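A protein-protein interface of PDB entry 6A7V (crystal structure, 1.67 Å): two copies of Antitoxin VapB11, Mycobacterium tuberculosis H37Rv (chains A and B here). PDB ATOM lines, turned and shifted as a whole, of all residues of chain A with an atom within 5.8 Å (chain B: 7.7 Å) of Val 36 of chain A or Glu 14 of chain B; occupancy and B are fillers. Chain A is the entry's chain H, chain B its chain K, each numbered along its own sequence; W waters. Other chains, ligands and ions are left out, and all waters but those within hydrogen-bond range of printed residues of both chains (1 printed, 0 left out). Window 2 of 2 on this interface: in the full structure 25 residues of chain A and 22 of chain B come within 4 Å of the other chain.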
ATOM      1  N   ALA A  31      19.979   8.208 -32.520  1.00  0.00           N
ATOM      2  CA  ALA A  31      19.312   7.010 -32.927  1.00  0.00           C
ATOM      3  C   ALA A  31      19.120   6.074 -31.721  1.00  0.00           C
ATOM      4  O   ALA A  31      18.105   5.415 -31.612  1.00  0.00           O
ATOM      5  CB  ALA A  31      20.085   6.306 -34.032  1.00  0.00           C
ATOM      6  N   LEU A  32      20.167   5.942 -30.908  1.00  0.00           N
ATOM      7  CA  LEU A  32      20.145   5.022 -29.813  1.00  0.00           C
ATOM      8  C   LEU A  32      19.335   5.597 -28.634  1.00  0.00           C
ATOM      9  O   LEU A  32      18.611   4.864 -27.975  1.00  0.00           O
ATOM     10  CB  LEU A  32      21.559   4.601 -29.386  1.00  0.00           C
ATOM     11  CG  LEU A  32      22.309   3.714 -30.391  1.00  0.00           C
ATOM     12  CD1 LEU A  32      23.701   3.396 -29.867  1.00  0.00           C
ATOM     13  CD2 LEU A  32      21.552   2.429 -30.705  1.00  0.00           C
ATOM     14  N   ARG A  33      19.527   6.859 -28.344  1.00  0.00           N
ATOM     15  CA  ARG A  33      18.846   7.486 -27.238  1.00  0.00           C
ATOM     16  C   ARG A  33      17.334   7.434 -27.422  1.00  0.00           C
ATOM     17  O   ARG A  33      16.610   7.169 -26.471  1.00  0.00           O
ATOM     18  CB  ARG A  33      19.308   8.948 -27.099  1.00  0.00           C
ATOM     19  CG  ARG A  33      18.700   9.710 -25.924  1.00  0.00           C
ATOM     20  CD  ARG A  33      18.712  11.221 -26.137  1.00  0.00           C
ATOM     21  NE  ARG A  33      17.602  11.884 -25.444  1.00  0.00           N
ATOM     22  CZ  ARG A  33      16.351  11.974 -25.905  1.00  0.00           C
ATOM     23  NH1 ARG A  33      15.425  12.598 -25.181  1.00  0.00           N
ATOM     24  NH2 ARG A  33      16.005  11.440 -27.076  1.00  0.00           N
ATOM     25  N   ARG A  34      16.885   7.697 -28.662  1.00  0.00           N
ATOM     26  CA  ARG A  34      15.484   7.700 -28.974  1.00  0.00           C
ATOM     27  C   ARG A  34      14.918   6.283 -28.681  1.00  0.00           C
ATOM     28  O   ARG A  34      13.812   6.159 -28.112  1.00  0.00           O
ATOM     29  CB  ARG A  34      15.185   8.087 -30.421  1.00  0.00           C
ATOM     30  CG  ARG A  34      13.700   7.967 -30.741  1.00  0.00           C
ATOM     31  CD  ARG A  34      13.337   8.444 -32.131  1.00  0.00           C
ATOM     32  NE  ARG A  34      13.330   9.900 -32.233  1.00  0.00           N
ATOM     33  CZ  ARG A  34      12.843  10.581 -33.269  1.00  0.00           C
ATOM     34  NH1 ARG A  34      12.309   9.949 -34.312  1.00  0.00           N
ATOM     35  NH2 ARG A  34      12.888  11.909 -33.262  1.00  0.00           N
ATOM     36  N   LEU A  35      15.648   5.224 -29.073  1.00  0.00           N
ATOM     37  CA  LEU A  35      15.056   3.938 -29.136  1.00  0.00           C
ATOM     38  C   LEU A  35      15.061   3.206 -27.805  1.00  0.00           C
ATOM     39  O   LEU A  35      14.117   2.504 -27.498  1.00  0.00           O
ATOM     40  CB  LEU A  35      15.783   3.095 -30.191  1.00  0.00           C
ATOM     41  CG  LEU A  35      15.169   1.747 -30.568  1.00  0.00           C
ATOM     42  CD1 LEU A  35      13.729   1.910 -31.034  1.00  0.00           C
ATOM     43  CD2 LEU A  35      16.018   1.086 -31.642  1.00  0.00           C
ATOM     44  N   VAL A  36      16.132   3.360 -27.031  1.00  0.00           N
ATOM     45  CA  VAL A  36      16.246   2.701 -25.725  1.00  0.00           C
ATOM     46  C   VAL A  36      16.627   3.655 -24.585  1.00  0.00           C
ATOM     47  O   VAL A  36      16.809   3.215 -23.451  1.00  0.00           O
ATOM     48  CB  VAL A  36      17.278   1.552 -25.768  1.00  0.00           C
ATOM     49  CG1 VAL A  36      16.784   0.411 -26.643  1.00  0.00           C
ATOM     50  CG2 VAL A  36      18.627   2.055 -26.255  1.00  0.00           C
ATOM     51  N   GLY A  37      16.741   4.950 -24.879  1.00  0.00           N
ATOM     52  CA  GLY A  37      17.110   5.934 -23.871  1.00  0.00           C
ATOM     53  C   GLY A  37      18.578   5.896 -23.499  1.00  0.00           C
ATOM     54  O   GLY A  37      19.424   5.434 -24.268  1.00  0.00           O
ATOM     55  N   SER A  38      18.867   6.406 -22.308  1.00  0.00           N
ATOM     56  CA  SER A  38      20.195   6.361 -21.724  1.00  0.00           C
ATOM     57  C   SER A  38      20.108   5.461 -20.504  1.00  0.00           C
ATOM     58  O   SER A  38      19.011   5.249 -19.979  1.00  0.00           O
ATOM     59  CB  SER A  38      20.647   7.762 -21.308  1.00  0.00           C
ATOM     60  OG  SER A  38      20.509   8.690 -22.372  1.00  0.00           O
ATOM     61  N   ASP B   8      28.225   2.820 -26.912  1.00  0.00           N
ATOM     62  CA  ASP B   8      28.021   2.227 -25.595  1.00  0.00           C
ATOM     63  C   ASP B   8      27.572   0.789 -25.779  1.00  0.00           C
ATOM     64  O   ASP B   8      26.625   0.522 -26.523  1.00  0.00           O
ATOM     65  CB  ASP B   8      26.971   3.003 -24.795  1.00  0.00           C
ATOM     66  CG  ASP B   8      26.867   2.529 -23.358  1.00  0.00           C
ATOM     67  OD1 ASP B   8      27.848   2.699 -22.604  1.00  0.00           O
ATOM     68  OD2 ASP B   8      25.807   1.990 -22.979  1.00  0.00           O
ATOM     69  N   ASP B   9      28.255  -0.133 -25.105  1.00  0.00           N
ATOM     70  CA  ASP B   9      28.008  -1.557 -25.301  1.00  0.00           C
ATOM     71  C   ASP B   9      26.565  -1.877 -24.904  1.00  0.00           C
ATOM     72  O   ASP B   9      25.861  -2.615 -25.627  1.00  0.00           O
ATOM     73  CB  ASP B   9      28.984  -2.410 -24.472  1.00  0.00           C
ATOM     74  CG  ASP B   9      30.413  -2.381 -25.013  1.00  0.00           C
ATOM     75  OD1 ASP B   9      30.639  -1.878 -26.133  1.00  0.00           O
ATOM     76  OD2 ASP B   9      31.321  -2.878 -24.311  1.00  0.00           O
ATOM     77  N   GLU B  10      26.106  -1.251 -23.814  1.00  0.00           N
ATOM     78  CA  GLU B  10      24.895  -1.647 -23.131  1.00  0.00           C
ATOM     79  C   GLU B  10      23.653  -1.179 -23.861  1.00  0.00           C
ATOM     80  O   GLU B  10      22.695  -1.972 -23.957  1.00  0.00           O
ATOM     81  CB  GLU B  10      24.885  -1.150 -21.678  1.00  0.00           C
ATOM     82  CG  GLU B  10      25.939  -1.806 -20.795  1.00  0.00           C
ATOM     83  CD  GLU B  10      25.846  -3.326 -20.790  1.00  0.00           C
ATOM     84  OE1 GLU B  10      24.716  -3.857 -20.713  1.00  0.00           O
ATOM     85  OE2 GLU B  10      26.899  -3.994 -20.873  1.00  0.00           O
ATOM     86  N   LEU B  11      23.709  -0.008 -24.479  1.00  0.00           N
ATOM     87  CA  LEU B  11      22.592   0.485 -25.273  1.00  0.00           C
ATOM     88  C   LEU B  11      22.347  -0.430 -26.482  1.00  0.00           C
ATOM     89  O   LEU B  11      21.213  -0.822 -26.782  1.00  0.00           O
ATOM     90  CB  LEU B  11      22.860   1.903 -25.782  1.00  0.00           C
ATOM     91  CG  LEU B  11      22.886   3.036 -24.758  1.00  0.00           C
ATOM     92  CD1 LEU B  11      23.225   4.345 -25.455  1.00  0.00           C
ATOM     93  CD2 LEU B  11      21.559   3.141 -24.022  1.00  0.00           C
ATOM     94  N   ALA B  12      23.436  -0.724 -27.190  1.00  0.00           N
ATOM     95  CA  ALA B  12      23.408  -1.630 -28.318  1.00  0.00           C
ATOM     96  C   ALA B  12      22.866  -2.987 -27.864  1.00  0.00           C
ATOM     97  O   ALA B  12      22.035  -3.564 -28.614  1.00  0.00           O
ATOM     98  CB  ALA B  12      24.798  -1.786 -28.919  1.00  0.00           C
ATOM     99  N   ALA B  13      23.306  -3.500 -26.728  1.00  0.00           N
ATOM    100  CA  ALA B  13      22.807  -4.768 -26.266  1.00  0.00           C
ATOM    101  C   ALA B  13      21.316  -4.757 -26.006  1.00  0.00           C
ATOM    102  O   ALA B  13      20.605  -5.681 -26.386  1.00  0.00           O
ATOM    103  CB  ALA B  13      23.551  -5.200 -25.010  1.00  0.00           C
ATOM    104  N   GLU B  14      20.844  -3.666 -25.425  1.00  0.00           N
ATOM    105  CA  GLU B  14      19.417  -3.455 -25.184  1.00  0.00           C
ATOM    106  C   GLU B  14      18.624  -3.467 -26.499  1.00  0.00           C
ATOM    107  O   GLU B  14      17.597  -4.116 -26.592  1.00  0.00           O
ATOM    108  CB  GLU B  14      19.174  -2.150 -24.415  1.00  0.00           C
ATOM    109  CG  GLU B  14      17.707  -1.823 -24.135  1.00  0.00           C
ATOM    110  CD  GLU B  14      16.988  -2.874 -23.303  1.00  0.00           C
ATOM    111  OE1 GLU B  14      17.655  -3.668 -22.601  1.00  0.00           O
ATOM    112  OE2 GLU B  14      15.738  -2.905 -23.348  1.00  0.00           O
ATOM    113  N   VAL B  15      19.173  -2.777 -27.496  1.00  0.00           N
ATOM    114  CA  VAL B  15      18.578  -2.717 -28.807  1.00  0.00           C
ATOM    115  C   VAL B  15      18.432  -4.148 -29.380  1.00  0.00           C
ATOM    116  O   VAL B  15      17.401  -4.537 -29.949  1.00  0.00           O
ATOM    117  CB  VAL B  15      19.319  -1.775 -29.785  1.00  0.00           C
ATOM    118  CG1 VAL B  15      18.755  -1.907 -31.194  1.00  0.00           C
ATOM    119  CG2 VAL B  15      19.180  -0.329 -29.328  1.00  0.00           C
ATOM    120  N   MET B  16      19.537  -4.884 -29.269  1.00  0.00           N
ATOM    121  CA  MET B  16      19.599  -6.246 -29.770  1.00  0.00           C
ATOM    122  C   MET B  16      18.539  -7.110 -29.116  1.00  0.00           C
ATOM    123  O   MET B  16      17.877  -7.900 -29.785  1.00  0.00           O
ATOM    124  CB  MET B  16      21.007  -6.831 -29.602  1.00  0.00           C
ATOM    125  CG  MET B  16      22.021  -6.214 -30.560  1.00  0.00           C
ATOM    126  SD  MET B  16      23.748  -6.505 -30.121  1.00  0.00           S
ATOM    127  CE  MET B  16      23.787  -8.297 -30.145  1.00  0.00           C
ATOM    128  N   ARG B  17      18.401  -6.957 -27.794  1.00  0.00           N
ATOM    129  CA  ARG B  17      17.436  -7.711 -27.021  1.00  0.00           C
ATOM    130  C   ARG B  17      15.985  -7.359 -27.474  1.00  0.00           C
ATOM    131  O   ARG B  17      15.169  -8.253 -27.760  1.00  0.00           O
ATOM    132  CB  ARG B  17      17.608  -7.462 -25.516  1.00  0.00           C
ATOM    133  CG  ARG B  17      17.328  -8.689 -24.661  1.00  0.00           C
ATOM    134  CD  ARG B  17      16.868  -8.328 -23.257  1.00  0.00           C
ATOM    135  NE  ARG B  17      15.431  -8.044 -23.225  1.00  0.00           N
ATOM    136  CZ  ARG B  17      14.874  -6.834 -23.141  1.00  0.00           C
ATOM    137  NH1 ARG B  17      13.551  -6.724 -23.126  1.00  0.00           N
ATOM    138  NH2 ARG B  17      15.614  -5.731 -23.065  1.00  0.00           N
ATOM    139  N   ARG B  18      15.708  -6.070 -27.601  1.00  0.00           N
ATOM    140  CA  ARG B  18      14.392  -5.647 -27.958  1.00  0.00           C
ATOM    141  C   ARG B  18      14.021  -6.038 -29.384  1.00  0.00           C
ATOM    142  O   ARG B  18      12.896  -6.516 -29.596  1.00  0.00           O
ATOM    143  CB  ARG B  18      14.242  -4.131 -27.786  1.00  0.00           C
ATOM    144  CG  ARG B  18      13.778  -3.699 -26.400  1.00  0.00           C
ATOM    145  CD  ARG B  18      13.223  -2.281 -26.426  1.00  0.00           C
ATOM    146  NE  ARG B  18      12.170  -2.131 -27.431  1.00  0.00           N
ATOM    147  CZ  ARG B  18      11.728  -0.970 -27.915  1.00  0.00           C
ATOM    148  NH1 ARG B  18      12.235   0.188 -27.496  1.00  0.00           N
ATOM    149  NH2 ARG B  18      10.767  -0.968 -28.832  1.00  0.00           N
ATOM    150  N   PHE B  19      14.946  -5.980 -30.334  1.00  0.00           N
ATOM    151  CA  PHE B  19      14.586  -6.282 -31.725  1.00  0.00           C
ATOM    152  C   PHE B  19      15.042  -7.633 -32.270  1.00  0.00           C
ATOM    153  O   PHE B  19      14.816  -7.929 -33.447  1.00  0.00           O
ATOM    154  CB  PHE B  19      15.045  -5.135 -32.612  1.00  0.00           C
ATOM    155  CG  PHE B  19      14.264  -3.888 -32.376  1.00  0.00           C
ATOM    156  CD1 PHE B  19      14.623  -3.013 -31.362  1.00  0.00           C
ATOM    157  CD2 PHE B  19      13.126  -3.625 -33.121  1.00  0.00           C
ATOM    158  CE1 PHE B  19      13.882  -1.875 -31.121  1.00  0.00           C
ATOM    159  CE2 PHE B  19      12.383  -2.489 -32.889  1.00  0.00           C
ATOM    160  CZ  PHE B  19      12.759  -1.616 -31.885  1.00  0.00           C
ATOM    161  N   GLY B  20      15.641  -8.463 -31.417  1.00  0.00           N
ATOM    162  CA  GLY B  20      16.036  -9.820 -31.812  1.00  0.00           C
ATOM    163  C   GLY B  20      17.138  -9.836 -32.855  1.00  0.00           C
ATOM    164  O   GLY B  20      17.118 -10.649 -33.782  1.00  0.00           O
ATOM    165  N   ALA B  27      21.966  -3.595 -35.125  1.00  0.00           N
ATOM    166  CA  ALA B  27      21.203  -2.846 -34.140  1.00  0.00           C
ATOM    167  C   ALA B  27      21.272  -1.344 -34.461  1.00  0.00           C
ATOM    168  O   ALA B  27      20.264  -0.618 -34.509  1.00  0.00           O
ATOM    169  CB  ALA B  27      21.739  -3.111 -32.740  1.00  0.00           C
ATOM    170  N   ALA B  31      18.426   1.302 -35.671  1.00  0.00           N
ATOM    171  CA  ALA B  31      18.154   2.525 -34.929  1.00  0.00           C
ATOM    172  C   ALA B  31      18.237   3.726 -35.886  1.00  0.00           C
ATOM    173  O   ALA B  31      17.417   4.617 -35.798  1.00  0.00           O
ATOM    174  CB  ALA B  31      19.125   2.676 -33.770  1.00  0.00           C
HETATM  175  O   HOH W   1      15.958   5.163 -33.393  1.00  0.00           O
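Of the 8 printed residues of chain A, 5 touch a printed residue of chain B. Printed residues of chain A that touch a printed residue of chain B: Ala 31, Leu 32, Leu 35, Val 36 and Gly 37. Hydrophobic or aromatic side chains of chain B within 4 Å of the printed part of chain A: Leu 11, Val 15, Phe 19 and Ala 31. Among the printed residues, 9 pairs touch across the chains. Among the printed residues, no Asp or Glu carboxylate lies within 4 Å of a Lys or Arg side-chain nitrogen of the other chain.
The side-chain carboxylate of Glu 14 of chain B is in salt-bridge range of the guanidinium group of Arg 17 of chain B. OD2 of Asp 8 of chain B is in hydrogen-bond range of N of Leu 11 of chain B (3.3 Å).
NH1 of Arg 18 of chain B lies within hydrogen-bond range of O of Leu 35 of chain A, 3.0 Å away.
O of Ala 31 of chain B touches CB of Ala 31 of chain A, 3.6 Å away. Leu 32 of chain A touches Val 15 of chain B. CB of Ala 31 of chain B touches CD2 of Leu 32 of chain A (3.9 Å). CD2 of Leu 35 of chain A touches CE1 of Phe 19 of chain B, at 3.7 Å. CG2 of Val 36 of chain A touches CD2 of Leu 11 of chain B, 3.8 Å away. Glu 14 of chain B touches Val 36 of chain A. Val 36 of chain A touches Val 15 of chain B (CG1 to CG2, 3.7 Å). O of Gly 37 of chain A touches CD2 of Leu 11 of chain B, 3.1 Å away.
Of the printed residues of chain B, Ala 31 of chain A touches Ala 31 (3.6 Å). Of the printed residues of chain B, Leu 32 of chain A touches Val 15 and Ala 31. Val 36 of chain A touches just these residues of chain B: Leu 11, Glu 14 and Val 15. Gly 37 of chain A touches just one residue of chain B: Leu 11. Of chain A, only Val 36 (3.5 Å) comes within 4 Å of Glu 14 of chain B. Printed residues of chain A within 4 Å of Val 15 of chain B: Leu 32 and Val 36. Of the printed residues of chain A, Phe 19 of chain B touches Leu 35. The nearest residue of chain B that does not touch Val 36 of chain A is Arg 18 of chain B (4.5 Å). The nearest printed residue of chain A that does not touch Glu 14 of chain B is Leu 35 of chain A (6.6 Å).
Water W1 bridges the backbone carbonyl oxygen (O) of Ala 31 of chain A (2.8 Å) and the backbone carbonyl oxygen (O) of Ala 31 of chain B (2.9 Å).
Ala 31 of chain A touches its own counterpart, Ala 31 of chain B.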
